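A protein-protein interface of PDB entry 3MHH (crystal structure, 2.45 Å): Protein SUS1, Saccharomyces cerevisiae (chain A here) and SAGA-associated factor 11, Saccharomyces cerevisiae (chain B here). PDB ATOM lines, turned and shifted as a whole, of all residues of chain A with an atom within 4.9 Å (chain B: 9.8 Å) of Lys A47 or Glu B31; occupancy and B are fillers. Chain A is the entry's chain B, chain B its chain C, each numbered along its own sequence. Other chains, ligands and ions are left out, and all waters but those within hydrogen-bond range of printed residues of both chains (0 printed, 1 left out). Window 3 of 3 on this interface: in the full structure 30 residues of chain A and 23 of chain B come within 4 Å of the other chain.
OE1 of Glu B31 lies within salt-bridge range of NZ of Lys A47 (2.8 Å).
The side-chain hydroxyl (OG1) of Thr B32 lies close to the backbone carbonyl oxygen (O) of Val B28 (3.3 Å).
The side-chain hydroxyl (OG1) of Thr B32 lies within hydrogen-bond range of the backbone carbonyl oxygen (O) of Ala B29 (3.3 Å).
Among the printed residues, pairs that only touch across the chains: Lys A43 with Ile B27, Lys A43 with Glu B31, Thr A46 with Val B28, Thr A46 with Glu B31, Met A50 with Thr B32 and Met A50 with Gln B35.
Of chain B, only Ile B27 (3.6 Å) and Glu B31 (3.7 Å) come within 4 Å of Lys A43.
Thr A46 touches two residues of chain B.
Lys A47 touches just one residue of chain B: Glu B31 (2.8 Å).
Of chain B, only Thr B32 and Gln B35 come within 4 Å of Met A50.
Of the printed residues of chain A, Ile B27 touches Lys A43 (3.6 Å).
Printed residues of chain A within 4 Å of Val B28: Thr A46 (3.6 Å).
Glu B31 touches just these residues of chain A: Lys A43, Thr A46 and Lys A47.
Of the printed residues of chain A, Thr B32 touches Met A50.
Of the printed residues of chain A, Gln B35 touches Met A50 (3.1 Å).
The nearest residue of chain B that does not touch Lys A47 is Gln B34 (5.6 Å).
The nearest printed residue of chain A that does not touch Val B28 is Met A50 (6.2 Å).
Printed residues of chain B that touch a printed residue of chain A: Ile B27, Val B28, Glu B31, Thr B32 and Gln B35.
Hydrophobic or aromatic side chains of chain B within 4 Å of the printed part of chain A: Ile B27 and Val B28.
Among the printed residues, Asp or Glu carboxylates within 4 Å of a Lys or Arg side-chain nitrogen of the other chain: Lys A47 with Glu B31.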
ATOM      1  N   LYS A  43     -24.386  20.238   6.809  1.00  0.00           N
ATOM      2  CA  LYS A  43     -24.256  21.211   7.886  1.00  0.00           C
ATOM      3  C   LYS A  43     -24.615  20.568   9.221  1.00  0.00           C
ATOM      4  O   LYS A  43     -23.914  20.756  10.216  1.00  0.00           O
ATOM      5  CB  LYS A  43     -25.142  22.428   7.626  1.00  0.00           C
ATOM      6  CG  LYS A  43     -24.714  23.227   6.398  1.00  0.00           C
ATOM      7  CD  LYS A  43     -25.549  24.487   6.212  1.00  0.00           C
ATOM      8  CE  LYS A  43     -25.214  25.187   4.900  1.00  0.00           C
ATOM      9  NZ  LYS A  43     -25.805  26.553   4.817  1.00  0.00           N
ATOM     10  N   ASP A  44     -25.697  19.801   9.240  1.00  0.00           N
ATOM     11  CA  ASP A  44     -26.097  19.103  10.457  1.00  0.00           C
ATOM     12  C   ASP A  44     -25.008  18.127  10.886  1.00  0.00           C
ATOM     13  O   ASP A  44     -24.614  18.075  12.053  1.00  0.00           O
ATOM     14  CB  ASP A  44     -27.399  18.331  10.228  1.00  0.00           C
ATOM     15  CG  ASP A  44     -28.600  19.243  10.052  1.00  0.00           C
ATOM     16  OD1 ASP A  44     -28.547  20.397  10.517  1.00  0.00           O
ATOM     17  OD2 ASP A  44     -29.615  18.790   9.473  1.00  0.00           O
ATOM     18  N   LEU A  45     -24.526  17.360   9.920  1.00  0.00           N
ATOM     19  CA  LEU A  45     -23.556  16.322  10.181  1.00  0.00           C
ATOM     20  C   LEU A  45     -22.288  16.926  10.739  1.00  0.00           C
ATOM     21  O   LEU A  45     -21.672  16.375  11.651  1.00  0.00           O
ATOM     22  CB  LEU A  45     -23.265  15.557   8.901  1.00  0.00           C
ATOM     23  CG  LEU A  45     -21.994  14.715   8.920  1.00  0.00           C
ATOM     24  CD1 LEU A  45     -22.018  13.679  10.052  1.00  0.00           C
ATOM     25  CD2 LEU A  45     -21.816  14.070   7.548  1.00  0.00           C
ATOM     26  N   THR A  46     -21.915  18.086  10.214  1.00  0.00           N
ATOM     27  CA  THR A  46     -20.749  18.802  10.714  1.00  0.00           C
ATOM     28  C   THR A  46     -20.970  19.265  12.153  1.00  0.00           C
ATOM     29  O   THR A  46     -20.123  19.038  13.021  1.00  0.00           O
ATOM     30  CB  THR A  46     -20.410  19.994   9.819  1.00  0.00           C
ATOM     31  OG1 THR A  46     -20.270  19.542   8.463  1.00  0.00           O
ATOM     32  CG2 THR A  46     -19.117  20.646  10.265  1.00  0.00           C
ATOM     33  N   LYS A  47     -22.111  19.896  12.417  1.00  0.00           N
ATOM     34  CA  LYS A  47     -22.421  20.332  13.774  1.00  0.00           C
ATOM     35  C   LYS A  47     -22.365  19.142  14.736  1.00  0.00           C
ATOM     36  O   LYS A  47     -21.853  19.243  15.851  1.00  0.00           O
ATOM     37  CB  LYS A  47     -23.807  20.982  13.838  1.00  0.00           C
ATOM     38  CG  LYS A  47     -23.835  22.425  13.355  1.00  0.00           C
ATOM     39  CD  LYS A  47     -25.198  23.064  13.576  1.00  0.00           C
ATOM     40  CE  LYS A  47     -25.231  24.506  13.074  1.00  0.00           C
ATOM     41  NZ  LYS A  47     -25.129  24.606  11.582  1.00  0.00           N
ATOM     42  N   SER A  48     -22.899  18.014  14.290  1.00  0.00           N
ATOM     43  CA  SER A  48     -22.973  16.829  15.120  1.00  0.00           C
ATOM     44  C   SER A  48     -21.571  16.316  15.380  1.00  0.00           C
ATOM     45  O   SER A  48     -21.254  15.889  16.483  1.00  0.00           O
ATOM     46  CB  SER A  48     -23.811  15.757  14.431  1.00  0.00           C
ATOM     47  OG  SER A  48     -23.647  14.508  15.065  1.00  0.00           O
ATOM     48  N   GLU A  49     -20.724  16.358  14.363  1.00  0.00           N
ATOM     49  CA  GLU A  49     -19.368  15.879  14.540  1.00  0.00           C
ATOM     50  C   GLU A  49     -18.571  16.800  15.451  1.00  0.00           C
ATOM     51  O   GLU A  49     -17.696  16.350  16.176  1.00  0.00           O
ATOM     52  CB  GLU A  49     -18.673  15.686  13.198  1.00  0.00           C
ATOM     53  CG  GLU A  49     -19.237  14.527  12.380  1.00  0.00           C
ATOM     54  CD  GLU A  49     -18.956  13.168  12.988  1.00  0.00           C
ATOM     55  OE1 GLU A  49     -18.225  13.099  14.003  1.00  0.00           O
ATOM     56  OE2 GLU A  49     -19.468  12.167  12.443  1.00  0.00           O
ATOM     57  N   MET A  50     -18.882  18.086  15.441  1.00  0.00           N
ATOM     58  CA  MET A  50     -18.203  19.004  16.348  1.00  0.00           C
ATOM     59  C   MET A  50     -18.515  18.625  17.794  1.00  0.00           C
ATOM     60  O   MET A  50     -17.607  18.459  18.609  1.00  0.00           O
ATOM     61  CB  MET A  50     -18.589  20.459  16.055  1.00  0.00           C
ATOM     62  CG  MET A  50     -17.864  21.009  14.836  1.00  0.00           C
ATOM     63  SD  MET A  50     -18.314  22.671  14.340  1.00  0.00           S
ATOM     64  CE  MET A  50     -17.177  23.627  15.314  1.00  0.00           C
ATOM     65  N   ASN A  51     -19.803  18.475  18.093  1.00  0.00           N
ATOM     66  CA  ASN A  51     -20.223  18.093  19.431  1.00  0.00           C
ATOM     67  C   ASN A  51     -19.641  16.739  19.840  1.00  0.00           C
ATOM     68  O   ASN A  51     -19.135  16.597  20.939  1.00  0.00           O
ATOM     69  CB  ASN A  51     -21.751  18.094  19.540  1.00  0.00           C
ATOM     70  CG  ASN A  51     -22.324  19.495  19.712  1.00  0.00           C
ATOM     71  OD1 ASN A  51     -21.676  20.379  20.279  1.00  0.00           O
ATOM     72  ND2 ASN A  51     -23.545  19.699  19.231  1.00  0.00           N
ATOM     73  N   LEU B  23     -16.915  21.544  -2.372  1.00  0.00           N
ATOM     74  CA  LEU B  23     -18.162  22.029  -1.812  1.00  0.00           C
ATOM     75  C   LEU B  23     -18.339  21.586  -0.354  1.00  0.00           C
ATOM     76  O   LEU B  23     -18.784  22.379   0.480  1.00  0.00           O
ATOM     77  CB  LEU B  23     -19.337  21.555  -2.652  1.00  0.00           C
ATOM     78  CG  LEU B  23     -20.715  21.988  -2.148  1.00  0.00           C
ATOM     79  CD1 LEU B  23     -20.835  23.529  -2.057  1.00  0.00           C
ATOM     80  CD2 LEU B  23     -21.792  21.391  -3.037  1.00  0.00           C
ATOM     81  N   ILE B  24     -18.012  20.325  -0.049  1.00  0.00           N
ATOM     82  CA  ILE B  24     -18.009  19.846   1.334  1.00  0.00           C
ATOM     83  C   ILE B  24     -17.058  20.686   2.213  1.00  0.00           C
ATOM     84  O   ILE B  24     -17.405  21.080   3.326  1.00  0.00           O
ATOM     85  CB  ILE B  24     -17.537  18.383   1.420  1.00  0.00           C
ATOM     86  CG1 ILE B  24     -18.557  17.427   0.777  1.00  0.00           C
ATOM     87  CG2 ILE B  24     -17.320  17.989   2.867  1.00  0.00           C
ATOM     88  CD1 ILE B  24     -17.978  16.027   0.496  1.00  0.00           C
ATOM     89  N   GLN B  25     -15.853  20.934   1.704  1.00  0.00           N
ATOM     90  CA  GLN B  25     -14.820  21.665   2.442  1.00  0.00           C
ATOM     91  C   GLN B  25     -15.162  23.128   2.643  1.00  0.00           C
ATOM     92  O   GLN B  25     -14.689  23.747   3.584  1.00  0.00           O
ATOM     93  CB  GLN B  25     -13.461  21.542   1.753  1.00  0.00           C
ATOM     94  CG  GLN B  25     -12.865  20.162   1.879  1.00  0.00           C
ATOM     95  CD  GLN B  25     -11.781  19.876   0.859  1.00  0.00           C
ATOM     96  OE1 GLN B  25     -10.982  20.747   0.520  1.00  0.00           O
ATOM     97  NE2 GLN B  25     -11.707  18.624   0.410  1.00  0.00           N
ATOM     98  N   ASP B  26     -15.976  23.673   1.750  1.00  0.00           N
ATOM     99  CA  ASP B  26     -16.500  25.024   1.889  1.00  0.00           C
ATOM    100  C   ASP B  26     -17.515  25.056   3.026  1.00  0.00           C
ATOM    101  O   ASP B  26     -17.416  25.887   3.934  1.00  0.00           O
ATOM    102  CB  ASP B  26     -17.187  25.441   0.586  1.00  0.00           C
ATOM    103  CG  ASP B  26     -17.730  26.841   0.631  1.00  0.00           C
ATOM    104  OD1 ASP B  26     -17.265  27.645   1.469  1.00  0.00           O
ATOM    105  OD2 ASP B  26     -18.606  27.148  -0.202  1.00  0.00           O
ATOM    106  N   ILE B  27     -18.480  24.132   2.980  1.00  0.00           N
ATOM    107  CA  ILE B  27     -19.533  24.054   3.985  1.00  0.00           C
ATOM    108  C   ILE B  27     -18.942  23.821   5.376  1.00  0.00           C
ATOM    109  O   ILE B  27     -19.280  24.515   6.342  1.00  0.00           O
ATOM    110  CB  ILE B  27     -20.535  22.932   3.649  1.00  0.00           C
ATOM    111  CG1 ILE B  27     -21.265  23.238   2.336  1.00  0.00           C
ATOM    112  CG2 ILE B  27     -21.567  22.770   4.763  1.00  0.00           C
ATOM    113  CD1 ILE B  27     -22.003  22.038   1.740  1.00  0.00           C
ATOM    114  N   VAL B  28     -18.025  22.877   5.478  1.00  0.00           N
ATOM    115  CA  VAL B  28     -17.435  22.573   6.766  1.00  0.00           C
ATOM    116  C   VAL B  28     -16.652  23.771   7.308  1.00  0.00           C
ATOM    117  O   VAL B  28     -16.727  24.074   8.496  1.00  0.00           O
ATOM    118  CB  VAL B  28     -16.549  21.320   6.696  1.00  0.00           C
ATOM    119  CG1 VAL B  28     -15.794  21.097   8.018  1.00  0.00           C
ATOM    120  CG2 VAL B  28     -17.404  20.095   6.335  1.00  0.00           C
ATOM    121  N   ALA B  29     -15.919  24.465   6.442  1.00  0.00           N
ATOM    122  CA  ALA B  29     -15.148  25.628   6.872  1.00  0.00           C
ATOM    123  C   ALA B  29     -16.077  26.693   7.465  1.00  0.00           C
ATOM    124  O   ALA B  29     -15.785  27.268   8.518  1.00  0.00           O
ATOM    125  CB  ALA B  29     -14.332  26.203   5.719  1.00  0.00           C
ATOM    126  N   ARG B  30     -17.205  26.925   6.802  1.00  0.00           N
ATOM    127  CA  ARG B  30     -18.174  27.908   7.265  1.00  0.00           C
ATOM    128  C   ARG B  30     -18.756  27.494   8.619  1.00  0.00           C
ATOM    129  O   ARG B  30     -19.016  28.330   9.484  1.00  0.00           O
ATOM    130  CB  ARG B  30     -19.296  28.075   6.233  1.00  0.00           C
ATOM    131  CG  ARG B  30     -18.843  28.733   4.931  1.00  0.00           C
ATOM    132  CD  ARG B  30     -20.020  28.981   3.980  1.00  0.00           C
ATOM    133  NE  ARG B  30     -19.598  29.125   2.584  1.00  0.00           N
ATOM    134  CZ  ARG B  30     -19.736  30.240   1.867  1.00  0.00           C
ATOM    135  NH1 ARG B  30     -20.297  31.311   2.407  1.00  0.00           N
ATOM    136  NH2 ARG B  30     -19.333  30.289   0.604  1.00  0.00           N
ATOM    137  N   GLU B  31     -18.928  26.190   8.798  1.00  0.00           N
ATOM    138  CA  GLU B  31     -19.462  25.643  10.040  1.00  0.00           C
ATOM    139  C   GLU B  31     -18.486  25.746  11.200  1.00  0.00           C
ATOM    140  O   GLU B  31     -18.859  26.182  12.290  1.00  0.00           O
ATOM    141  CB  GLU B  31     -19.834  24.177   9.842  1.00  0.00           C
ATOM    142  CG  GLU B  31     -21.079  23.998   9.026  1.00  0.00           C
ATOM    143  CD  GLU B  31     -22.282  24.561   9.716  1.00  0.00           C
ATOM    144  OE1 GLU B  31     -22.400  24.360  10.947  1.00  0.00           O
ATOM    145  OE2 GLU B  31     -23.110  25.191   9.032  1.00  0.00           O
ATOM    146  N   THR B  32     -17.248  25.317  10.969  1.00  0.00           N
ATOM    147  CA  THR B  32     -16.235  25.283  12.030  1.00  0.00           C
ATOM    148  C   THR B  32     -15.815  26.684  12.471  1.00  0.00           C
ATOM    149  O   THR B  32     -15.543  26.903  13.643  1.00  0.00           O
ATOM    150  CB  THR B  32     -14.983  24.471  11.624  1.00  0.00           C
ATOM    151  OG1 THR B  32     -14.332  25.081  10.501  1.00  0.00           O
ATOM    152  CG2 THR B  32     -15.363  23.043  11.270  1.00  0.00           C
ATOM    153  N   THR B  33     -15.803  27.637  11.544  1.00  0.00           N
ATOM    154  CA  THR B  33     -15.460  29.022  11.877  1.00  0.00           C
ATOM    155  C   THR B  33     -16.575  29.677  12.690  1.00  0.00           C
ATOM    156  O   THR B  33     -16.310  30.446  13.601  1.00  0.00           O
ATOM    157  CB  THR B  33     -15.208  29.873  10.612  1.00  0.00           C
ATOM    158  OG1 THR B  33     -16.343  29.799   9.755  1.00  0.00           O
ATOM    159  CG2 THR B  33     -13.985  29.386   9.854  1.00  0.00           C
ATOM    160  N   GLN B  34     -17.820  29.361  12.370  1.00  0.00           N
ATOM    161  CA  GLN B  34     -18.956  29.948  13.086  1.00  0.00           C
ATOM    162  C   GLN B  34     -18.996  29.484  14.533  1.00  0.00           C
ATOM    163  O   GLN B  34     -19.180  30.284  15.458  1.00  0.00           O
ATOM    164  CB  GLN B  34     -20.274  29.575  12.404  1.00  0.00           C
ATOM    165  CG  GLN B  34     -20.569  30.355  11.141  1.00  0.00           C
ATOM    166  CD  GLN B  34     -21.871  29.931  10.452  1.00  0.00           C
ATOM    167  OE1 GLN B  34     -21.912  29.781   9.235  1.00  0.00           O
ATOM    168  NE2 GLN B  34     -22.933  29.756  11.228  1.00  0.00           N
ATOM    169  N   GLN B  35     -18.838  28.179  14.725  1.00  0.00           N
ATOM    170  CA  GLN B  35     -18.944  27.583  16.048  1.00  0.00           C
ATOM    171  C   GLN B  35     -17.742  28.010  16.879  1.00  0.00           C
ATOM    172  O   GLN B  35     -17.895  28.361  18.052  1.00  0.00           O
ATOM    173  CB  GLN B  35     -19.055  26.055  15.935  1.00  0.00           C
ATOM    174  CG  GLN B  35     -19.334  25.320  17.224  1.00  0.00           C
ATOM    175  CD  GLN B  35     -20.664  25.682  17.873  1.00  0.00           C
ATOM    176  OE1 GLN B  35     -21.488  26.410  17.307  1.00  0.00           O
ATOM    177  NE2 GLN B  35     -20.883  25.154  19.075  1.00  0.00           N
ATOM    178  N   GLN B  36     -16.559  28.022  16.266  1.00  0.00           N
ATOM    179  CA  GLN B  36     -15.361  28.516  16.954  1.00  0.00           C
ATOM    180  C   GLN B  36     -15.605  29.946  17.433  1.00  0.00           C
ATOM    181  O   GLN B  36     -15.222  30.300  18.543  1.00  0.00           O
ATOM    182  CB  GLN B  36     -14.101  28.465  16.073  1.00  0.00           C
ATOM    183  CG  GLN B  36     -12.830  28.822  16.847  1.00  0.00           C
ATOM    184  CD  GLN B  36     -11.659  29.309  15.984  1.00  0.00           C
ATOM    185  OE1 GLN B  36     -11.829  30.077  15.030  1.00  0.00           O
ATOM    186  NE2 GLN B  36     -10.446  28.899  16.365  1.00  0.00           N
ATOM    187  N   LEU B  37     -16.269  30.752  16.608  1.00  0.00           N
ATOM    188  CA  LEU B  37     -16.614  32.112  17.006  1.00  0.00           C
ATOM    189  C   LEU B  37     -17.583  32.117  18.180  1.00  0.00           C
ATOM    190  O   LEU B  37     -17.317  32.736  19.197  1.00  0.00           O
ATOM    191  CB  LEU B  37     -17.190  32.909  15.837  1.00  0.00           C
ATOM    192  CG  LEU B  37     -17.589  34.349  16.168  1.00  0.00           C
ATOM    193  CD1 LEU B  37     -16.412  35.144  16.690  1.00  0.00           C
ATOM    194  CD2 LEU B  37     -18.198  35.046  14.946  1.00  0.00           C
ATOM    195  N   LEU B  38     -18.706  31.419  18.052  1.00  0.00           N
ATOM    196  CA  LEU B  38     -19.684  31.374  19.143  1.00  0.00           C
ATOM    197  C   LEU B  38     -19.036  30.953  20.467  1.00  0.00           C
ATOM    198  O   LEU B  38     -19.326  31.533  21.518  1.00  0.00           O
ATOM    199  CB  LEU B  38     -20.815  30.408  18.809  1.00  0.00           C
ATOM    200  CG  LEU B  38     -21.786  30.856  17.726  1.00  0.00           C
ATOM    201  CD1 LEU B  38     -22.830  29.779  17.482  1.00  0.00           C
ATOM    202  CD2 LEU B  38     -22.452  32.161  18.096  1.00  0.00           C
ATOM    203  N   LYS B  39     -18.161  29.945  20.409  1.00  0.00           N
ATOM    204  CA  LYS B  39     -17.580  29.351  21.618  1.00  0.00           C
ATOM    205  C   LYS B  39     -16.546  30.268  22.268  1.00  0.00           C
ATOM    206  O   LYS B  39     -16.452  30.334  23.491  1.00  0.00           O
ATOM    207  CB  LYS B  39     -16.946  27.984  21.316  1.00  0.00           C
ATOM    208  CG  LYS B  39     -17.942  26.851  21.022  1.00  0.00           C
ATOM    209  CD  LYS B  39     -17.295  25.465  21.245  1.00  0.00           C
ATOM    210  CE  LYS B  39     -18.063  24.334  20.539  1.00  0.00           C
ATOM    211  NZ  LYS B  39     -17.301  23.028  20.519  1.00  0.00           N
ATOM    212  N   SER B  47     -27.022  25.585  24.337  1.00  0.00           N
ATOM    213  CA  SER B  47     -27.921  25.378  23.213  1.00  0.00           C
ATOM    214  C   SER B  47     -29.341  25.764  23.621  1.00  0.00           C
ATOM    215  O   SER B  47     -29.654  25.844  24.806  1.00  0.00           O
ATOM    216  CB  SER B  47     -27.923  23.913  22.796  1.00  0.00           C
ATOM    217  OG  SER B  47     -29.138  23.306  23.201  1.00  0.00           O
